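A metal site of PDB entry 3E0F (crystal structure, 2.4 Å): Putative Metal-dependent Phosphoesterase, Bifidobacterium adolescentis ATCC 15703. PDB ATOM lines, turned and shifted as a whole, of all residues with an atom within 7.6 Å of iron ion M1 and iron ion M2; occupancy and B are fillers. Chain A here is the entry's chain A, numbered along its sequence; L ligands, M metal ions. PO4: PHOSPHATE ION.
O of Ala 48 lies close to ND1 of His 20 (3.2 Å).
OD1 of Asp 261 sits close to NZ of Lys 267, at 3.8 Å.
The backbone carbonyl oxygen (O) of His 18 is in hydrogen-bond range of the backbone NH (N) of Trp 262, at 3.4 Å.
The backbone NH (N) of His 203 lies within hydrogen-bond range of the side-chain carboxylate (OE1) of Glu 231, 3.0 Å away.
The backbone carbonyl oxygen (O) of Asp 261 is in hydrogen-bond range of a ring nitrogen (ND1) of His 263.
N of His 20 lies within hydrogen-bond range of O of Trp 262, at 2.8 Å.
The backbone NH (N) of Glu 75 is in hydrogen-bond range of the backbone carbonyl oxygen (O) of Asp 49 (3.0 Å).
OD2 of Asp 261 sits at hydrogen-bond distance from NE2 of His 234.
Within 4 Å of iron ion M1: Glu 75, His 86 and His 203.
Within 4 Å of iron ion M2: His 18, His 20, Glu 75 and Asp 261.
The nearest printed residue that does not touch iron ion M2 is His 263 (4.2 Å).
O2 of the ligand binds iron ion M1 (2.0 Å).
Iron ion M1 is bound by the side-chain carboxylate (OE2) of Glu 75 (2.0 Å).
ND1 of His 86 binds iron ion M1, 2.2 Å away.
A ring nitrogen (NE2) of His 203 binds iron ion M1 (2.5 Å).
Iron ion M2 is bound by an oxygen (O4) of the ligand (2.0 Å), the side-chain carboxylate (OE1) of Glu 75 (2.1 Å), a ring nitrogen (NE2) of His 18 (2.2 Å), a ring nitrogen (NE2) of His 20 (2.3 Å) and the side-chain carboxylate (OD1) of Asp 261 (2.4 Å).
Iron ion M2 has five donor atoms within binding distance.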
ATOM      1  N   HIS A  18       0.557   9.426 -20.383  1.00  0.00           N
ATOM      2  CA  HIS A  18       0.897  10.844 -20.525  1.00  0.00           C
ATOM      3  C   HIS A  18       2.271  11.185 -19.852  1.00  0.00           C
ATOM      4  O   HIS A  18       2.363  11.682 -18.734  1.00  0.00           O
ATOM      5  CB  HIS A  18      -0.272  11.652 -19.923  1.00  0.00           C
ATOM      6  CG  HIS A  18      -0.253  13.102 -20.254  1.00  0.00           C
ATOM      7  ND1 HIS A  18      -1.337  13.926 -20.012  1.00  0.00           N
ATOM      8  CD2 HIS A  18       0.709  13.893 -20.798  1.00  0.00           C
ATOM      9  CE1 HIS A  18      -1.030  15.154 -20.390  1.00  0.00           C
ATOM     10  NE2 HIS A  18       0.197  15.169 -20.855  1.00  0.00           N
ATOM     11  N   CYS A  19       3.352  10.907 -20.584  1.00  0.00           N
ATOM     12  CA  CYS A  19       4.713  11.048 -20.060  1.00  0.00           C
ATOM     13  C   CYS A  19       5.595  11.747 -21.067  1.00  0.00           C
ATOM     14  O   CYS A  19       5.542  11.447 -22.237  1.00  0.00           O
ATOM     15  CB  CYS A  19       5.303   9.671 -19.780  1.00  0.00           C
ATOM     16  SG  CYS A  19       4.277   8.545 -18.844  1.00  0.00           S
ATOM     17  N   HIS A  20       6.394  12.692 -20.600  1.00  0.00           N
ATOM     18  CA  HIS A  20       7.299  13.467 -21.416  1.00  0.00           C
ATOM     19  C   HIS A  20       8.771  13.070 -21.187  1.00  0.00           C
ATOM     20  O   HIS A  20       9.162  12.694 -20.070  1.00  0.00           O
ATOM     21  CB  HIS A  20       7.094  14.928 -21.081  1.00  0.00           C
ATOM     22  CG  HIS A  20       5.708  15.404 -21.373  1.00  0.00           C
ATOM     23  ND1 HIS A  20       5.352  15.932 -22.587  1.00  0.00           N
ATOM     24  CD2 HIS A  20       4.577  15.384 -20.630  1.00  0.00           C
ATOM     25  CE1 HIS A  20       4.067  16.233 -22.579  1.00  0.00           C
ATOM     26  NE2 HIS A  20       3.580  15.921 -21.397  1.00  0.00           N
ATOM     27  N   ASP A  25       9.943  18.371 -23.125  1.00  0.00           N
ATOM     28  CA  ASP A  25      10.304  19.088 -21.899  1.00  0.00           C
ATOM     29  C   ASP A  25      10.418  18.232 -20.652  1.00  0.00           C
ATOM     30  O   ASP A  25      10.430  18.758 -19.549  1.00  0.00           O
ATOM     31  CB  ASP A  25       9.315  20.216 -21.630  1.00  0.00           C
ATOM     32  CG  ASP A  25       7.863  19.728 -21.544  1.00  0.00           C
ATOM     33  OD1 ASP A  25       7.609  18.528 -21.764  1.00  0.00           O
ATOM     34  OD2 ASP A  25       6.977  20.570 -21.282  1.00  0.00           O
ATOM     35  N   ALA A  48       4.417  10.832 -24.822  1.00  0.00           N
ATOM     36  CA  ALA A  48       3.437  11.896 -25.178  1.00  0.00           C
ATOM     37  C   ALA A  48       4.117  13.270 -25.282  1.00  0.00           C
ATOM     38  O   ALA A  48       3.667  14.255 -24.678  1.00  0.00           O
ATOM     39  CB  ALA A  48       2.262  11.924 -24.172  1.00  0.00           C
ATOM     40  N   ASP A  49       5.180  13.326 -26.064  1.00  0.00           N
ATOM     41  CA  ASP A  49       5.987  14.535 -26.154  1.00  0.00           C
ATOM     42  C   ASP A  49       5.258  15.565 -26.979  1.00  0.00           C
ATOM     43  O   ASP A  49       4.504  15.219 -27.853  1.00  0.00           O
ATOM     44  CB  ASP A  49       7.402  14.252 -26.731  1.00  0.00           C
ATOM     45  CG  ASP A  49       8.343  13.578 -25.709  1.00  0.00           C
ATOM     46  OD1 ASP A  49       8.421  14.049 -24.555  1.00  0.00           O
ATOM     47  OD2 ASP A  49       9.006  12.579 -26.069  1.00  0.00           O
ATOM     48  N   HIS A  50       5.507  16.839 -26.662  1.00  0.00           N
ATOM     49  CA  HIS A  50       4.934  17.949 -27.391  1.00  0.00           C
ATOM     50  C   HIS A  50       5.315  17.979 -28.841  1.00  0.00           C
ATOM     51  O   HIS A  50       6.501  18.058 -29.162  1.00  0.00           O
ATOM     52  CB  HIS A  50       5.336  19.287 -26.790  1.00  0.00           C
ATOM     53  CG  HIS A  50       4.912  19.460 -25.385  1.00  0.00           C
ATOM     54  ND1 HIS A  50       3.598  19.681 -25.033  1.00  0.00           N
ATOM     55  CD2 HIS A  50       5.608  19.401 -24.229  1.00  0.00           C
ATOM     56  CE1 HIS A  50       3.511  19.799 -23.720  1.00  0.00           C
ATOM     57  NE2 HIS A  50       4.715  19.633 -23.207  1.00  0.00           N
ATOM     58  N   GLU A  75       1.575  14.927 -27.472  1.00  0.00           N
ATOM     59  CA  GLU A  75       0.699  15.957 -26.954  1.00  0.00           C
ATOM     60  C   GLU A  75       0.774  17.170 -27.893  1.00  0.00           C
ATOM     61  O   GLU A  75       1.836  17.696 -28.181  1.00  0.00           O
ATOM     62  CB  GLU A  75       1.100  16.369 -25.530  1.00  0.00           C
ATOM     63  CG  GLU A  75       0.165  17.411 -24.947  1.00  0.00           C
ATOM     64  CD  GLU A  75       0.344  17.672 -23.477  1.00  0.00           C
ATOM     65  OE1 GLU A  75       1.290  17.153 -22.874  1.00  0.00           O
ATOM     66  OE2 GLU A  75      -0.476  18.446 -22.908  1.00  0.00           O
ATOM     67  N   ILE A  76      -0.393  17.593 -28.386  1.00  0.00           N
ATOM     68  CA  ILE A  76      -0.498  18.650 -29.372  1.00  0.00           C
ATOM     69  C   ILE A  76      -1.167  19.825 -28.695  1.00  0.00           C
ATOM     70  O   ILE A  76      -2.243  19.688 -28.111  1.00  0.00           O
ATOM     71  CB  ILE A  76      -1.334  18.209 -30.607  1.00  0.00           C
ATOM     72  CG1 ILE A  76      -0.839  16.864 -31.119  1.00  0.00           C
ATOM     73  CG2 ILE A  76      -1.254  19.255 -31.696  1.00  0.00           C
ATOM     74  CD1 ILE A  76      -1.771  16.181 -32.151  1.00  0.00           C
ATOM     75  N   THR A  77      -0.538  21.001 -28.725  1.00  0.00           N
ATOM     76  CA  THR A  77      -1.216  22.204 -28.234  1.00  0.00           C
ATOM     77  C   THR A  77      -2.142  22.720 -29.321  1.00  0.00           C
ATOM     78  O   THR A  77      -1.787  22.772 -30.490  1.00  0.00           O
ATOM     79  CB  THR A  77      -0.260  23.343 -27.800  1.00  0.00           C
ATOM     80  OG1 THR A  77       0.803  22.800 -26.998  1.00  0.00           O
ATOM     81  CG2 THR A  77      -1.050  24.430 -27.015  1.00  0.00           C
ATOM     82  N   VAL A  85      -5.929  24.394 -25.325  1.00  0.00           N
ATOM     83  CA  VAL A  85      -6.342  22.996 -25.170  1.00  0.00           C
ATOM     84  C   VAL A  85      -5.185  22.057 -25.546  1.00  0.00           C
ATOM     85  O   VAL A  85      -4.540  22.231 -26.577  1.00  0.00           O
ATOM     86  CB  VAL A  85      -7.562  22.621 -26.098  1.00  0.00           C
ATOM     87  CG1 VAL A  85      -8.066  21.232 -25.779  1.00  0.00           C
ATOM     88  CG2 VAL A  85      -8.672  23.621 -25.951  1.00  0.00           C
ATOM     89  N   HIS A  86      -4.904  21.067 -24.706  1.00  0.00           N
ATOM     90  CA  HIS A  86      -3.861  20.118 -25.060  1.00  0.00           C
ATOM     91  C   HIS A  86      -4.516  18.787 -25.418  1.00  0.00           C
ATOM     92  O   HIS A  86      -5.457  18.344 -24.746  1.00  0.00           O
ATOM     93  CB  HIS A  86      -2.875  19.932 -23.920  1.00  0.00           C
ATOM     94  CG  HIS A  86      -2.094  21.157 -23.567  1.00  0.00           C
ATOM     95  ND1 HIS A  86      -0.985  21.122 -22.739  1.00  0.00           N
ATOM     96  CD2 HIS A  86      -2.223  22.447 -23.951  1.00  0.00           C
ATOM     97  CE1 HIS A  86      -0.500  22.340 -22.607  1.00  0.00           C
ATOM     98  NE2 HIS A  86      -1.231  23.161 -23.335  1.00  0.00           N
ATOM     99  N   MET A  87      -4.016  18.149 -26.456  1.00  0.00           N
ATOM    100  CA  MET A  87      -4.607  16.943 -26.962  1.00  0.00           C
ATOM    101  C   MET A  87      -3.582  15.847 -27.037  1.00  0.00           C
ATOM    102  O   MET A  87      -2.487  16.031 -27.551  1.00  0.00           O
ATOM    103  CB  MET A  87      -5.173  17.201 -28.338  1.00  0.00           C
ATOM    104  CG  MET A  87      -5.879  18.545 -28.402  1.00  0.00           C
ATOM    105  SD  MET A  87      -7.561  18.394 -29.264  1.00  0.00           S
ATOM    106  CE  MET A  87      -8.528  17.542 -27.837  1.00  0.00           C
ATOM    107  N   LEU A  88      -3.942  14.691 -26.499  1.00  0.00           N
ATOM    108  CA  LEU A  88      -3.111  13.524 -26.611  1.00  0.00           C
ATOM    109  C   LEU A  88      -3.537  12.795 -27.886  1.00  0.00           C
ATOM    110  O   LEU A  88      -4.719  12.528 -28.102  1.00  0.00           O
ATOM    111  CB  LEU A  88      -3.268  12.648 -25.371  1.00  0.00           C
ATOM    112  CG  LEU A  88      -2.968  13.355 -24.058  1.00  0.00           C
ATOM    113  CD1 LEU A  88      -3.373  12.490 -22.850  1.00  0.00           C
ATOM    114  CD2 LEU A  88      -1.498  13.725 -24.001  1.00  0.00           C
ATOM    115  N   ALA A 202      -6.669  16.459 -23.193  1.00  0.00           N
ATOM    116  CA  ALA A 202      -5.823  16.344 -22.008  1.00  0.00           C
ATOM    117  C   ALA A 202      -6.228  17.393 -20.977  1.00  0.00           C
ATOM    118  O   ALA A 202      -6.475  18.541 -21.337  1.00  0.00           O
ATOM    119  CB  ALA A 202      -4.310  16.547 -22.403  1.00  0.00           C
ATOM    120  N   HIS A 203      -6.249  16.976 -19.694  1.00  0.00           N
ATOM    121  CA  HIS A 203      -6.562  17.834 -18.527  1.00  0.00           C
ATOM    122  C   HIS A 203      -7.548  18.993 -18.786  1.00  0.00           C
ATOM    123  O   HIS A 203      -7.244  20.144 -18.465  1.00  0.00           O
ATOM    124  CB  HIS A 203      -5.261  18.368 -17.898  1.00  0.00           C
ATOM    125  CG  HIS A 203      -4.355  19.069 -18.857  1.00  0.00           C
ATOM    126  ND1 HIS A 203      -4.627  20.316 -19.375  1.00  0.00           N
ATOM    127  CD2 HIS A 203      -3.147  18.702 -19.364  1.00  0.00           C
ATOM    128  CE1 HIS A 203      -3.636  20.692 -20.175  1.00  0.00           C
ATOM    129  NE2 HIS A 203      -2.735  19.721 -20.186  1.00  0.00           N
ATOM    130  N   ASP A 206      -8.500  21.541 -15.988  1.00  0.00           N
ATOM    131  CA  ASP A 206      -7.393  22.247 -15.318  1.00  0.00           C
ATOM    132  C   ASP A 206      -7.406  23.795 -15.591  1.00  0.00           C
ATOM    133  O   ASP A 206      -7.104  24.236 -16.708  1.00  0.00           O
ATOM    134  CB  ASP A 206      -6.061  21.600 -15.752  1.00  0.00           C
ATOM    135  CG  ASP A 206      -4.859  22.075 -14.959  1.00  0.00           C
ATOM    136  OD1 ASP A 206      -4.960  23.016 -14.145  1.00  0.00           O
ATOM    137  OD2 ASP A 206      -3.770  21.481 -15.149  1.00  0.00           O
ATOM    138  N   GLU A 231      -9.155  12.970 -20.810  1.00  0.00           N
ATOM    139  CA  GLU A 231      -8.289  12.613 -19.701  1.00  0.00           C
ATOM    140  C   GLU A 231      -8.963  13.144 -18.440  1.00  0.00           C
ATOM    141  O   GLU A 231      -9.050  14.335 -18.231  1.00  0.00           O
ATOM    142  CB  GLU A 231      -6.897  13.199 -19.904  1.00  0.00           C
ATOM    143  CG  GLU A 231      -5.847  12.794 -18.880  1.00  0.00           C
ATOM    144  CD  GLU A 231      -4.462  13.391 -19.193  1.00  0.00           C
ATOM    145  OE1 GLU A 231      -4.381  14.614 -19.373  1.00  0.00           O
ATOM    146  OE2 GLU A 231      -3.463  12.639 -19.257  1.00  0.00           O
ATOM    147  N   HIS A 234      -6.165  13.081 -13.745  1.00  0.00           N
ATOM    148  CA  HIS A 234      -5.002  13.923 -13.898  1.00  0.00           C
ATOM    149  C   HIS A 234      -5.019  14.891 -12.723  1.00  0.00           C
ATOM    150  O   HIS A 234      -6.079  15.374 -12.311  1.00  0.00           O
ATOM    151  CB  HIS A 234      -5.103  14.674 -15.214  1.00  0.00           C
ATOM    152  CG  HIS A 234      -3.911  15.524 -15.526  1.00  0.00           C
ATOM    153  ND1 HIS A 234      -3.677  16.721 -14.899  1.00  0.00           N
ATOM    154  CD2 HIS A 234      -2.934  15.373 -16.430  1.00  0.00           C
ATOM    155  CE1 HIS A 234      -2.581  17.250 -15.377  1.00  0.00           C
ATOM    156  NE2 HIS A 234      -2.117  16.470 -16.323  1.00  0.00           N
ATOM    157  N   SER A 260       0.111  10.681 -15.690  1.00  0.00           N
ATOM    158  CA  SER A 260       0.830  11.426 -14.676  1.00  0.00           C
ATOM    159  C   SER A 260       1.225  12.799 -15.162  1.00  0.00           C
ATOM    160  O   SER A 260       1.339  13.704 -14.366  1.00  0.00           O
ATOM    161  CB  SER A 260       2.072  10.687 -14.269  1.00  0.00           C
ATOM    162  OG  SER A 260       2.967  10.593 -15.350  1.00  0.00           O
ATOM    163  N   ASP A 261       1.431  12.973 -16.473  1.00  0.00           N
ATOM    164  CA  ASP A 261       2.000  14.200 -17.016  1.00  0.00           C
ATOM    165  C   ASP A 261       3.442  14.397 -16.510  1.00  0.00           C
ATOM    166  O   ASP A 261       3.922  15.500 -16.296  1.00  0.00           O
ATOM    167  CB  ASP A 261       1.121  15.392 -16.685  1.00  0.00           C
ATOM    168  CG  ASP A 261       1.064  16.351 -17.773  1.00  0.00           C
ATOM    169  OD1 ASP A 261       2.000  16.348 -18.566  1.00  0.00           O
ATOM    170  OD2 ASP A 261       0.084  17.092 -17.859  1.00  0.00           O
ATOM    171  N   TRP A 262       4.092  13.268 -16.315  1.00  0.00           N
ATOM    172  CA  TRP A 262       5.424  13.197 -15.810  1.00  0.00           C
ATOM    173  C   TRP A 262       6.345  13.926 -16.736  1.00  0.00           C
ATOM    174  O   TRP A 262       6.313  13.715 -17.950  1.00  0.00           O
ATOM    175  CB  TRP A 262       5.830  11.745 -15.814  1.00  0.00           C
ATOM    176  CG  TRP A 262       7.159  11.402 -15.269  1.00  0.00           C
ATOM    177  CD1 TRP A 262       7.558  11.463 -13.958  1.00  0.00           C
ATOM    178  CD2 TRP A 262       8.243  10.811 -15.997  1.00  0.00           C
ATOM    179  NE1 TRP A 262       8.836  10.976 -13.847  1.00  0.00           N
ATOM    180  CE2 TRP A 262       9.269  10.556 -15.077  1.00  0.00           C
ATOM    181  CE3 TRP A 262       8.434  10.473 -17.339  1.00  0.00           C
ATOM    182  CZ2 TRP A 262      10.469   9.999 -15.452  1.00  0.00           C
ATOM    183  CZ3 TRP A 262       9.614   9.920 -17.708  1.00  0.00           C
ATOM    184  CH2 TRP A 262      10.628   9.691 -16.780  1.00  0.00           C
ATOM    185  N   HIS A 263       7.192  14.759 -16.136  1.00  0.00           N
ATOM    186  CA  HIS A 263       8.262  15.395 -16.844  1.00  0.00           C
ATOM    187  C   HIS A 263       9.563  15.057 -16.159  1.00  0.00           C
ATOM    188  O   HIS A 263      10.524  15.797 -16.278  1.00  0.00           O
ATOM    189  CB  HIS A 263       8.065  16.909 -16.842  1.00  0.00           C
ATOM    190  CG  HIS A 263       6.954  17.367 -17.721  1.00  0.00           C
ATOM    191  ND1 HIS A 263       5.638  17.053 -17.489  1.00  0.00           N
ATOM    192  CD2 HIS A 263       6.967  18.136 -18.824  1.00  0.00           C
ATOM    193  CE1 HIS A 263       4.891  17.606 -18.410  1.00  0.00           C
ATOM    194  NE2 HIS A 263       5.671  18.269 -19.231  1.00  0.00           N
ATOM    195  N   LYS A 267       8.966  18.485 -13.039  1.00  0.00           N
ATOM    196  CA  LYS A 267       7.668  18.658 -12.388  1.00  0.00           C
ATOM    197  C   LYS A 267       7.595  17.749 -11.164  1.00  0.00           C
ATOM    198  O   LYS A 267       8.278  16.726 -11.112  1.00  0.00           O
ATOM    199  CB  LYS A 267       6.510  18.245 -13.321  1.00  0.00           C
ATOM    200  CG  LYS A 267       6.249  19.144 -14.532  1.00  0.00           C
ATOM    201  CD  LYS A 267       4.955  19.894 -14.441  1.00  0.00           C
ATOM    202  CE  LYS A 267       4.300  20.116 -15.824  1.00  0.00           C
ATOM    203  NZ  LYS A 267       3.350  18.991 -16.230  1.00  0.00           N
ATOM    204  N   ASN A 269       5.016  15.904 -10.549  1.00  0.00           N
ATOM    205  CA  ASN A 269       4.189  14.771 -10.967  1.00  0.00           C
ATOM    206  C   ASN A 269       4.979  13.499 -11.042  1.00  0.00           C
ATOM    207  O   ASN A 269       6.037  13.469 -11.667  1.00  0.00           O
ATOM    208  CB  ASN A 269       3.568  14.980 -12.372  1.00  0.00           C
ATOM    209  CG  ASN A 269       2.833  16.286 -12.512  1.00  0.00           C
ATOM    210  OD1 ASN A 269       3.208  17.284 -11.896  1.00  0.00           O
ATOM    211  ND2 ASN A 269       1.807  16.301 -13.352  1.00  0.00           N
HETATM  212  P   PO4 L   1       2.372  20.011 -20.156  1.00  0.00           P
HETATM  213  O1  PO4 L   1       1.963  19.899 -18.691  1.00  0.00           O
HETATM  214  O2  PO4 L   1       1.279  20.492 -21.100  1.00  0.00           O
HETATM  215  O3  PO4 L   1       3.570  20.937 -20.211  1.00  0.00           O
HETATM  216  O4  PO4 L   1       2.658  18.613 -20.671  1.00  0.00           O
HETATM  217 FE    FE M   1      -0.522  19.623 -21.243  1.00  0.00          FE
HETATM  218 FE    FE M   2       1.571  16.900 -20.826  1.00  0.00          FE
HETATM  219 ZN    ZN M   3       5.114  19.516 -21.110  1.00  0.00          ZN
